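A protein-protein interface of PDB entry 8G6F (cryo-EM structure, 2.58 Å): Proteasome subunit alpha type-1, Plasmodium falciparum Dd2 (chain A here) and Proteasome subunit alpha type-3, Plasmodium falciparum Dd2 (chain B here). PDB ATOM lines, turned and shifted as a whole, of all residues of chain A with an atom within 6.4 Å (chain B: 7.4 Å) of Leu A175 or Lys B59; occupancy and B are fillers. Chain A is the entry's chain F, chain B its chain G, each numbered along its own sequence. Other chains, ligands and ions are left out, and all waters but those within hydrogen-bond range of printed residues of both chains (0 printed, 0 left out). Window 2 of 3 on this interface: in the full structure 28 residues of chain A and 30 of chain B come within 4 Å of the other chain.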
ATOM      1  N   ASP A 156     -12.077   9.581  26.727  1.00  0.00           N
ATOM      2  CA  ASP A 156     -12.583   9.021  27.972  1.00  0.00           C
ATOM      3  C   ASP A 156     -12.858   7.531  27.843  1.00  0.00           C
ATOM      4  O   ASP A 156     -12.668   6.782  28.807  1.00  0.00           O
ATOM      5  CB  ASP A 156     -13.862   9.745  28.399  1.00  0.00           C
ATOM      6  CG  ASP A 156     -13.594  11.143  28.918  1.00  0.00           C
ATOM      7  OD1 ASP A 156     -12.595  11.332  29.641  1.00  0.00           O
ATOM      8  OD2 ASP A 156     -14.387  12.056  28.606  1.00  0.00           O
ATOM      9  N   ALA A 157     -13.313   7.098  26.673  1.00  0.00           N
ATOM     10  CA  ALA A 157     -13.384   5.694  26.312  1.00  0.00           C
ATOM     11  C   ALA A 157     -13.016   5.580  24.844  1.00  0.00           C
ATOM     12  O   ALA A 157     -13.256   6.501  24.061  1.00  0.00           O
ATOM     13  CB  ALA A 157     -14.772   5.106  26.565  1.00  0.00           C
ATOM     14  N   TYR A 170     -21.870   0.518  22.637  1.00  0.00           N
ATOM     15  CA  TYR A 170     -21.984   0.205  24.058  1.00  0.00           C
ATOM     16  C   TYR A 170     -21.327   1.283  24.914  1.00  0.00           C
ATOM     17  O   TYR A 170     -21.877   1.697  25.943  1.00  0.00           O
ATOM     18  CB  TYR A 170     -21.360  -1.160  24.340  1.00  0.00           C
ATOM     19  CG  TYR A 170     -21.352  -1.543  25.800  1.00  0.00           C
ATOM     20  CD1 TYR A 170     -22.405  -2.247  26.358  1.00  0.00           C
ATOM     21  CD2 TYR A 170     -20.290  -1.200  26.619  1.00  0.00           C
ATOM     22  CE1 TYR A 170     -22.400  -2.594  27.688  1.00  0.00           C
ATOM     23  CE2 TYR A 170     -20.278  -1.543  27.947  1.00  0.00           C
ATOM     24  CZ  TYR A 170     -21.332  -2.241  28.477  1.00  0.00           C
ATOM     25  OH  TYR A 170     -21.318  -2.582  29.804  1.00  0.00           O
ATOM     26  N   LEU A 171     -20.142   1.740  24.510  1.00  0.00           N
ATOM     27  CA  LEU A 171     -19.448   2.771  25.272  1.00  0.00           C
ATOM     28  C   LEU A 171     -20.229   4.075  25.270  1.00  0.00           C
ATOM     29  O   LEU A 171     -20.333   4.744  26.301  1.00  0.00           O
ATOM     30  CB  LEU A 171     -18.046   2.989  24.706  1.00  0.00           C
ATOM     31  CG  LEU A 171     -17.052   1.837  24.854  1.00  0.00           C
ATOM     32  CD1 LEU A 171     -15.732   2.211  24.219  1.00  0.00           C
ATOM     33  CD2 LEU A 171     -16.855   1.461  26.311  1.00  0.00           C
ATOM     34  N   GLU A 172     -20.776   4.467  24.121  1.00  0.00           N
ATOM     35  CA  GLU A 172     -21.571   5.686  24.077  1.00  0.00           C
ATOM     36  C   GLU A 172     -22.815   5.560  24.940  1.00  0.00           C
ATOM     37  O   GLU A 172     -23.293   6.558  25.490  1.00  0.00           O
ATOM     38  CB  GLU A 172     -21.950   6.012  22.636  1.00  0.00           C
ATOM     39  CG  GLU A 172     -20.773   6.442  21.783  1.00  0.00           C
ATOM     40  CD  GLU A 172     -21.162   6.701  20.345  1.00  0.00           C
ATOM     41  OE1 GLU A 172     -22.204   6.174  19.903  1.00  0.00           O
ATOM     42  OE2 GLU A 172     -20.425   7.431  19.653  1.00  0.00           O
ATOM     43  N   LYS A 173     -23.356   4.349  25.067  1.00  0.00           N
ATOM     44  CA  LYS A 173     -24.516   4.155  25.929  1.00  0.00           C
ATOM     45  C   LYS A 173     -24.144   4.268  27.404  1.00  0.00           C
ATOM     46  O   LYS A 173     -24.870   4.894  28.183  1.00  0.00           O
ATOM     47  CB  LYS A 173     -25.156   2.798  25.641  1.00  0.00           C
ATOM     48  CG  LYS A 173     -26.663   2.774  25.831  1.00  0.00           C
ATOM     49  CD  LYS A 173     -27.194   1.352  25.937  1.00  0.00           C
ATOM     50  CE  LYS A 173     -26.959   0.763  27.320  1.00  0.00           C
ATOM     51  NZ  LYS A 173     -26.895  -0.726  27.293  1.00  0.00           N
ATOM     52  N   ASN A 174     -23.021   3.676  27.807  1.00  0.00           N
ATOM     53  CA  ASN A 174     -22.674   3.552  29.219  1.00  0.00           C
ATOM     54  C   ASN A 174     -21.610   4.542  29.681  1.00  0.00           C
ATOM     55  O   ASN A 174     -21.088   4.392  30.788  1.00  0.00           O
ATOM     56  CB  ASN A 174     -22.199   2.128  29.516  1.00  0.00           C
ATOM     57  CG  ASN A 174     -23.291   1.101  29.333  1.00  0.00           C
ATOM     58  OD1 ASN A 174     -23.942   0.698  30.293  1.00  0.00           O
ATOM     59  ND2 ASN A 174     -23.498   0.673  28.097  1.00  0.00           N
ATOM     60  N   LEU A 175     -21.275   5.547  28.872  1.00  0.00           N
ATOM     61  CA  LEU A 175     -20.169   6.435  29.222  1.00  0.00           C
ATOM     62  C   LEU A 175     -20.400   7.140  30.550  1.00  0.00           C
ATOM     63  O   LEU A 175     -19.470   7.286  31.350  1.00  0.00           O
ATOM     64  CB  LEU A 175     -19.952   7.457  28.109  1.00  0.00           C
ATOM     65  CG  LEU A 175     -18.822   8.465  28.331  1.00  0.00           C
ATOM     66  CD1 LEU A 175     -17.507   7.763  28.631  1.00  0.00           C
ATOM     67  CD2 LEU A 175     -18.684   9.369  27.118  1.00  0.00           C
ATOM     68  N   HIS A 176     -21.627   7.595  30.804  1.00  0.00           N
ATOM     69  CA  HIS A 176     -21.879   8.376  32.008  1.00  0.00           C
ATOM     70  C   HIS A 176     -21.631   7.581  33.282  1.00  0.00           C
ATOM     71  O   HIS A 176     -21.496   8.177  34.354  1.00  0.00           O
ATOM     72  CB  HIS A 176     -23.313   8.906  31.999  1.00  0.00           C
ATOM     73  CG  HIS A 176     -24.349   7.837  31.850  1.00  0.00           C
ATOM     74  ND1 HIS A 176     -24.738   7.344  30.624  1.00  0.00           N
ATOM     75  CD2 HIS A 176     -25.078   7.168  32.773  1.00  0.00           C
ATOM     76  CE1 HIS A 176     -25.661   6.416  30.798  1.00  0.00           C
ATOM     77  NE2 HIS A 176     -25.885   6.290  32.094  1.00  0.00           N
ATOM     78  N   LEU A 177     -21.564   6.254  33.195  1.00  0.00           N
ATOM     79  CA  LEU A 177     -21.401   5.418  34.375  1.00  0.00           C
ATOM     80  C   LEU A 177     -19.948   5.156  34.742  1.00  0.00           C
ATOM     81  O   LEU A 177     -19.676   4.772  35.883  1.00  0.00           O
ATOM     82  CB  LEU A 177     -22.101   4.073  34.163  1.00  0.00           C
ATOM     83  CG  LEU A 177     -23.567   4.147  33.747  1.00  0.00           C
ATOM     84  CD1 LEU A 177     -24.073   2.771  33.352  1.00  0.00           C
ATOM     85  CD2 LEU A 177     -24.409   4.727  34.869  1.00  0.00           C
ATOM     86  N   PHE A 178     -19.014   5.355  33.812  1.00  0.00           N
ATOM     87  CA  PHE A 178     -17.643   4.908  34.037  1.00  0.00           C
ATOM     88  C   PHE A 178     -16.927   5.767  35.071  1.00  0.00           C
ATOM     89  O   PHE A 178     -16.100   5.260  35.837  1.00  0.00           O
ATOM     90  CB  PHE A 178     -16.871   4.910  32.718  1.00  0.00           C
ATOM     91  CG  PHE A 178     -17.463   4.018  31.662  1.00  0.00           C
ATOM     92  CD1 PHE A 178     -18.224   2.915  32.006  1.00  0.00           C
ATOM     93  CD2 PHE A 178     -17.249   4.280  30.325  1.00  0.00           C
ATOM     94  CE1 PHE A 178     -18.761   2.100  31.034  1.00  0.00           C
ATOM     95  CE2 PHE A 178     -17.786   3.467  29.351  1.00  0.00           C
ATOM     96  CZ  PHE A 178     -18.542   2.376  29.707  1.00  0.00           C
ATOM     97  N   GLU A 179     -17.226   7.065  35.114  1.00  0.00           N
ATOM     98  CA  GLU A 179     -16.437   7.974  35.941  1.00  0.00           C
ATOM     99  C   GLU A 179     -16.489   7.577  37.412  1.00  0.00           C
ATOM    100  O   GLU A 179     -15.463   7.592  38.101  1.00  0.00           O
ATOM    101  CB  GLU A 179     -16.928   9.408  35.748  1.00  0.00           C
ATOM    102  CG  GLU A 179     -16.328  10.432  36.707  1.00  0.00           C
ATOM    103  CD  GLU A 179     -14.867  10.709  36.430  1.00  0.00           C
ATOM    104  OE1 GLU A 179     -14.415  10.443  35.296  1.00  0.00           O
ATOM    105  OE2 GLU A 179     -14.171  11.200  37.342  1.00  0.00           O
ATOM    106  N   MET B  55     -15.471  17.351  14.741  1.00  0.00           N
ATOM    107  CA  MET B  55     -15.530  16.335  15.783  1.00  0.00           C
ATOM    108  C   MET B  55     -16.872  16.325  16.504  1.00  0.00           C
ATOM    109  O   MET B  55     -16.956  15.891  17.656  1.00  0.00           O
ATOM    110  CB  MET B  55     -14.394  16.549  16.778  1.00  0.00           C
ATOM    111  CG  MET B  55     -13.026  16.222  16.220  1.00  0.00           C
ATOM    112  SD  MET B  55     -11.744  17.288  16.890  1.00  0.00           S
ATOM    113  CE  MET B  55     -11.042  16.194  18.119  1.00  0.00           C
ATOM    114  N   ASP B  56     -17.930  16.797  15.845  1.00  0.00           N
ATOM    115  CA  ASP B  56     -19.254  16.784  16.451  1.00  0.00           C
ATOM    116  C   ASP B  56     -19.820  15.379  16.596  1.00  0.00           C
ATOM    117  O   ASP B  56     -20.838  15.213  17.273  1.00  0.00           O
ATOM    118  CB  ASP B  56     -20.219  17.636  15.624  1.00  0.00           C
ATOM    119  CG  ASP B  56     -20.245  17.237  14.162  1.00  0.00           C
ATOM    120  OD1 ASP B  56     -19.244  16.665  13.684  1.00  0.00           O
ATOM    121  OD2 ASP B  56     -21.265  17.491  13.491  1.00  0.00           O
ATOM    122  N   LYS B  57     -19.200  14.376  15.976  1.00  0.00           N
ATOM    123  CA  LYS B  57     -19.658  12.996  16.060  1.00  0.00           C
ATOM    124  C   LYS B  57     -18.710  12.114  16.862  1.00  0.00           C
ATOM    125  O   LYS B  57     -18.884  10.891  16.884  1.00  0.00           O
ATOM    126  CB  LYS B  57     -19.847  12.419  14.656  1.00  0.00           C
ATOM    127  CG  LYS B  57     -20.826  13.193  13.788  1.00  0.00           C
ATOM    128  CD  LYS B  57     -22.248  13.112  14.323  1.00  0.00           C
ATOM    129  CE  LYS B  57     -22.820  14.495  14.580  1.00  0.00           C
ATOM    130  NZ  LYS B  57     -24.200  14.445  15.131  1.00  0.00           N
ATOM    131  N   ASN B  58     -17.713  12.698  17.515  1.00  0.00           N
ATOM    132  CA  ASN B  58     -16.781  11.973  18.371  1.00  0.00           C
ATOM    133  C   ASN B  58     -17.174  12.285  19.813  1.00  0.00           C
ATOM    134  O   ASN B  58     -16.641  13.205  20.434  1.00  0.00           O
ATOM    135  CB  ASN B  58     -15.344  12.370  18.069  1.00  0.00           C
ATOM    136  CG  ASN B  58     -14.369  11.246  18.312  1.00  0.00           C
ATOM    137  OD1 ASN B  58     -14.631  10.342  19.102  1.00  0.00           O
ATOM    138  ND2 ASN B  58     -13.231  11.293  17.632  1.00  0.00           N
ATOM    139  N   LYS B  59     -18.117  11.511  20.341  1.00  0.00           N
ATOM    140  CA  LYS B  59     -18.708  11.786  21.641  1.00  0.00           C
ATOM    141  C   LYS B  59     -17.895  11.230  22.801  1.00  0.00           C
ATOM    142  O   LYS B  59     -18.245  11.480  23.958  1.00  0.00           O
ATOM    143  CB  LYS B  59     -20.129  11.221  21.699  1.00  0.00           C
ATOM    144  CG  LYS B  59     -20.992  11.579  20.500  1.00  0.00           C
ATOM    145  CD  LYS B  59     -20.990  13.077  20.229  1.00  0.00           C
ATOM    146  CE  LYS B  59     -22.336  13.567  19.706  1.00  0.00           C
ATOM    147  NZ  LYS B  59     -23.070  14.382  20.711  1.00  0.00           N
ATOM    148  N   MET B  60     -16.826  10.488  22.525  1.00  0.00           N
ATOM    149  CA  MET B  60     -15.993   9.900  23.564  1.00  0.00           C
ATOM    150  C   MET B  60     -14.648  10.604  23.700  1.00  0.00           C
ATOM    151  O   MET B  60     -13.777  10.118  24.424  1.00  0.00           O
ATOM    152  CB  MET B  60     -15.792   8.413  23.277  1.00  0.00           C
ATOM    153  CG  MET B  60     -16.928   7.539  23.800  1.00  0.00           C
ATOM    154  SD  MET B  60     -17.190   5.966  22.954  1.00  0.00           S
ATOM    155  CE  MET B  60     -15.698   5.760  21.983  1.00  0.00           C
ATOM    156  N   ILE B  61     -14.463  11.735  23.032  1.00  0.00           N
ATOM    157  CA  ILE B  61     -13.239  12.515  23.163  1.00  0.00           C
ATOM    158  C   ILE B  61     -13.266  13.266  24.484  1.00  0.00           C
ATOM    159  O   ILE B  61     -14.295  13.822  24.880  1.00  0.00           O
ATOM    160  CB  ILE B  61     -13.089  13.482  21.976  1.00  0.00           C
ATOM    161  CG1 ILE B  61     -12.566  12.739  20.750  1.00  0.00           C
ATOM    162  CG2 ILE B  61     -12.157  14.628  22.328  1.00  0.00           C
ATOM    163  CD1 ILE B  61     -11.075  12.561  20.734  1.00  0.00           C
ATOM    164  N   LYS B  62     -12.131  13.282  25.176  1.00  0.00           N
ATOM    165  CA  LYS B  62     -12.038  14.014  26.430  1.00  0.00           C
ATOM    166  C   LYS B  62     -12.344  15.487  26.197  1.00  0.00           C
ATOM    167  O   LYS B  62     -11.823  16.101  25.263  1.00  0.00           O
ATOM    168  CB  LYS B  62     -10.648  13.848  27.035  1.00  0.00           C
ATOM    169  CG  LYS B  62     -10.559  14.282  28.477  1.00  0.00           C
ATOM    170  CD  LYS B  62      -9.145  14.196  28.993  1.00  0.00           C
ATOM    171  CE  LYS B  62      -9.006  14.906  30.323  1.00  0.00           C
ATOM    172  NZ  LYS B  62      -7.585  15.124  30.697  1.00  0.00           N
ATOM    173  N   LYS B  63     -13.189  16.055  27.053  1.00  0.00           N
ATOM    174  CA  LYS B  63     -13.700  17.398  26.819  1.00  0.00           C
ATOM    175  C   LYS B  63     -12.569  18.417  26.813  1.00  0.00           C
ATOM    176  O   LYS B  63     -11.723  18.433  27.710  1.00  0.00           O
ATOM    177  CB  LYS B  63     -14.727  17.765  27.889  1.00  0.00           C
ATOM    178  CG  LYS B  63     -15.910  16.809  27.974  1.00  0.00           C
ATOM    179  CD  LYS B  63     -16.890  17.013  26.830  1.00  0.00           C
ATOM    180  CE  LYS B  63     -16.755  15.929  25.776  1.00  0.00           C
ATOM    181  NZ  LYS B  63     -17.917  15.897  24.847  1.00  0.00           N
ATOM    182  N   ASN B 211     -23.118  21.966  22.024  1.00  0.00           N
ATOM    183  CA  ASN B 211     -21.724  21.629  21.771  1.00  0.00           C
ATOM    184  C   ASN B 211     -20.829  22.853  21.630  1.00  0.00           C
ATOM    185  O   ASN B 211     -19.643  22.704  21.321  1.00  0.00           O
ATOM    186  CB  ASN B 211     -21.611  20.752  20.522  1.00  0.00           C
ATOM    187  CG  ASN B 211     -22.032  21.470  19.256  1.00  0.00           C
ATOM    188  OD1 ASN B 211     -22.283  22.672  19.261  1.00  0.00           O
ATOM    189  ND2 ASN B 211     -22.107  20.728  18.159  1.00  0.00           N
ATOM    190  N   ASN B 214     -17.674  22.736  24.184  1.00  0.00           N
ATOM    191  CA  ASN B 214     -16.658  21.694  24.143  1.00  0.00           C
ATOM    192  C   ASN B 214     -16.008  21.524  22.777  1.00  0.00           C
ATOM    193  O   ASN B 214     -15.096  20.702  22.647  1.00  0.00           O
ATOM    194  CB  ASN B 214     -17.253  20.354  24.596  1.00  0.00           C
ATOM    195  CG  ASN B 214     -18.518  20.000  23.859  1.00  0.00           C
ATOM    196  OD1 ASN B 214     -18.988  20.754  23.011  1.00  0.00           O
ATOM    197  ND2 ASN B 214     -19.087  18.849  24.185  1.00  0.00           N
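Among the printed residues, pairs that only touch across the chains: Ala A157 with Met B60 (3.3 Å), Leu A171 with Met B60 (3.6 Å), Asp A156 with Lys B62 (3.8 Å), Glu A172 with Met B60 (3.8 Å) and Leu A175 with Lys B59 (3.8 Å).
Of the 12 printed residues of chain A, 5 touch a printed residue of chain B.
Printed residues of chain A that touch a printed residue of chain B: Asp A156, Ala A157, Leu A171, Glu A172 and Leu A175.
Hydrophobic or aromatic side chains of chain A within 4 Å of the printed part of chain B: Leu A171 and Leu A175.
Of the 11 printed residues of chain B, 3 touch a printed residue of chain A.
Hydrophobic or aromatic side chains of chain B within 4 Å of the printed part of chain A: Met B60.
Among the printed residues, 6 pairs touch across the chains.
Among the printed residues, no Asp or Glu carboxylate lies within 4 Å of a Lys or Arg side-chain nitrogen of the other chain.
Leu A175 touches just one residue of chain B: Lys B59 (3.8 Å).
Lys B59 touches just one residue of chain A: Leu A175 (3.8 Å).
Of the printed residues of chain B, Leu A171 touches Met B60 (3.6 Å).
Of the printed residues of chain B, Glu A172 touches Met B60 (3.8 Å).
Printed residues of chain A within 4 Å of Met B60: Asp A156 (2.9 Å), Ala A157 (3.3 Å), Leu A171 (3.6 Å) and Glu A172 (3.8 Å).
Of the printed residues of chain B, Asp A156 touches Met B60 and Lys B62.
Printed residues of chain B within 4 Å of Ala A157: Met B60 (3.3 Å).
The nearest printed residue of chain B that does not touch Glu A172 is Lys B59 (4.3 Å).
The backbone NH (N) of Asp A156 sits at hydrogen-bond distance from the backbone carbonyl oxygen (O) of Met B60, at 2.9 Å.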
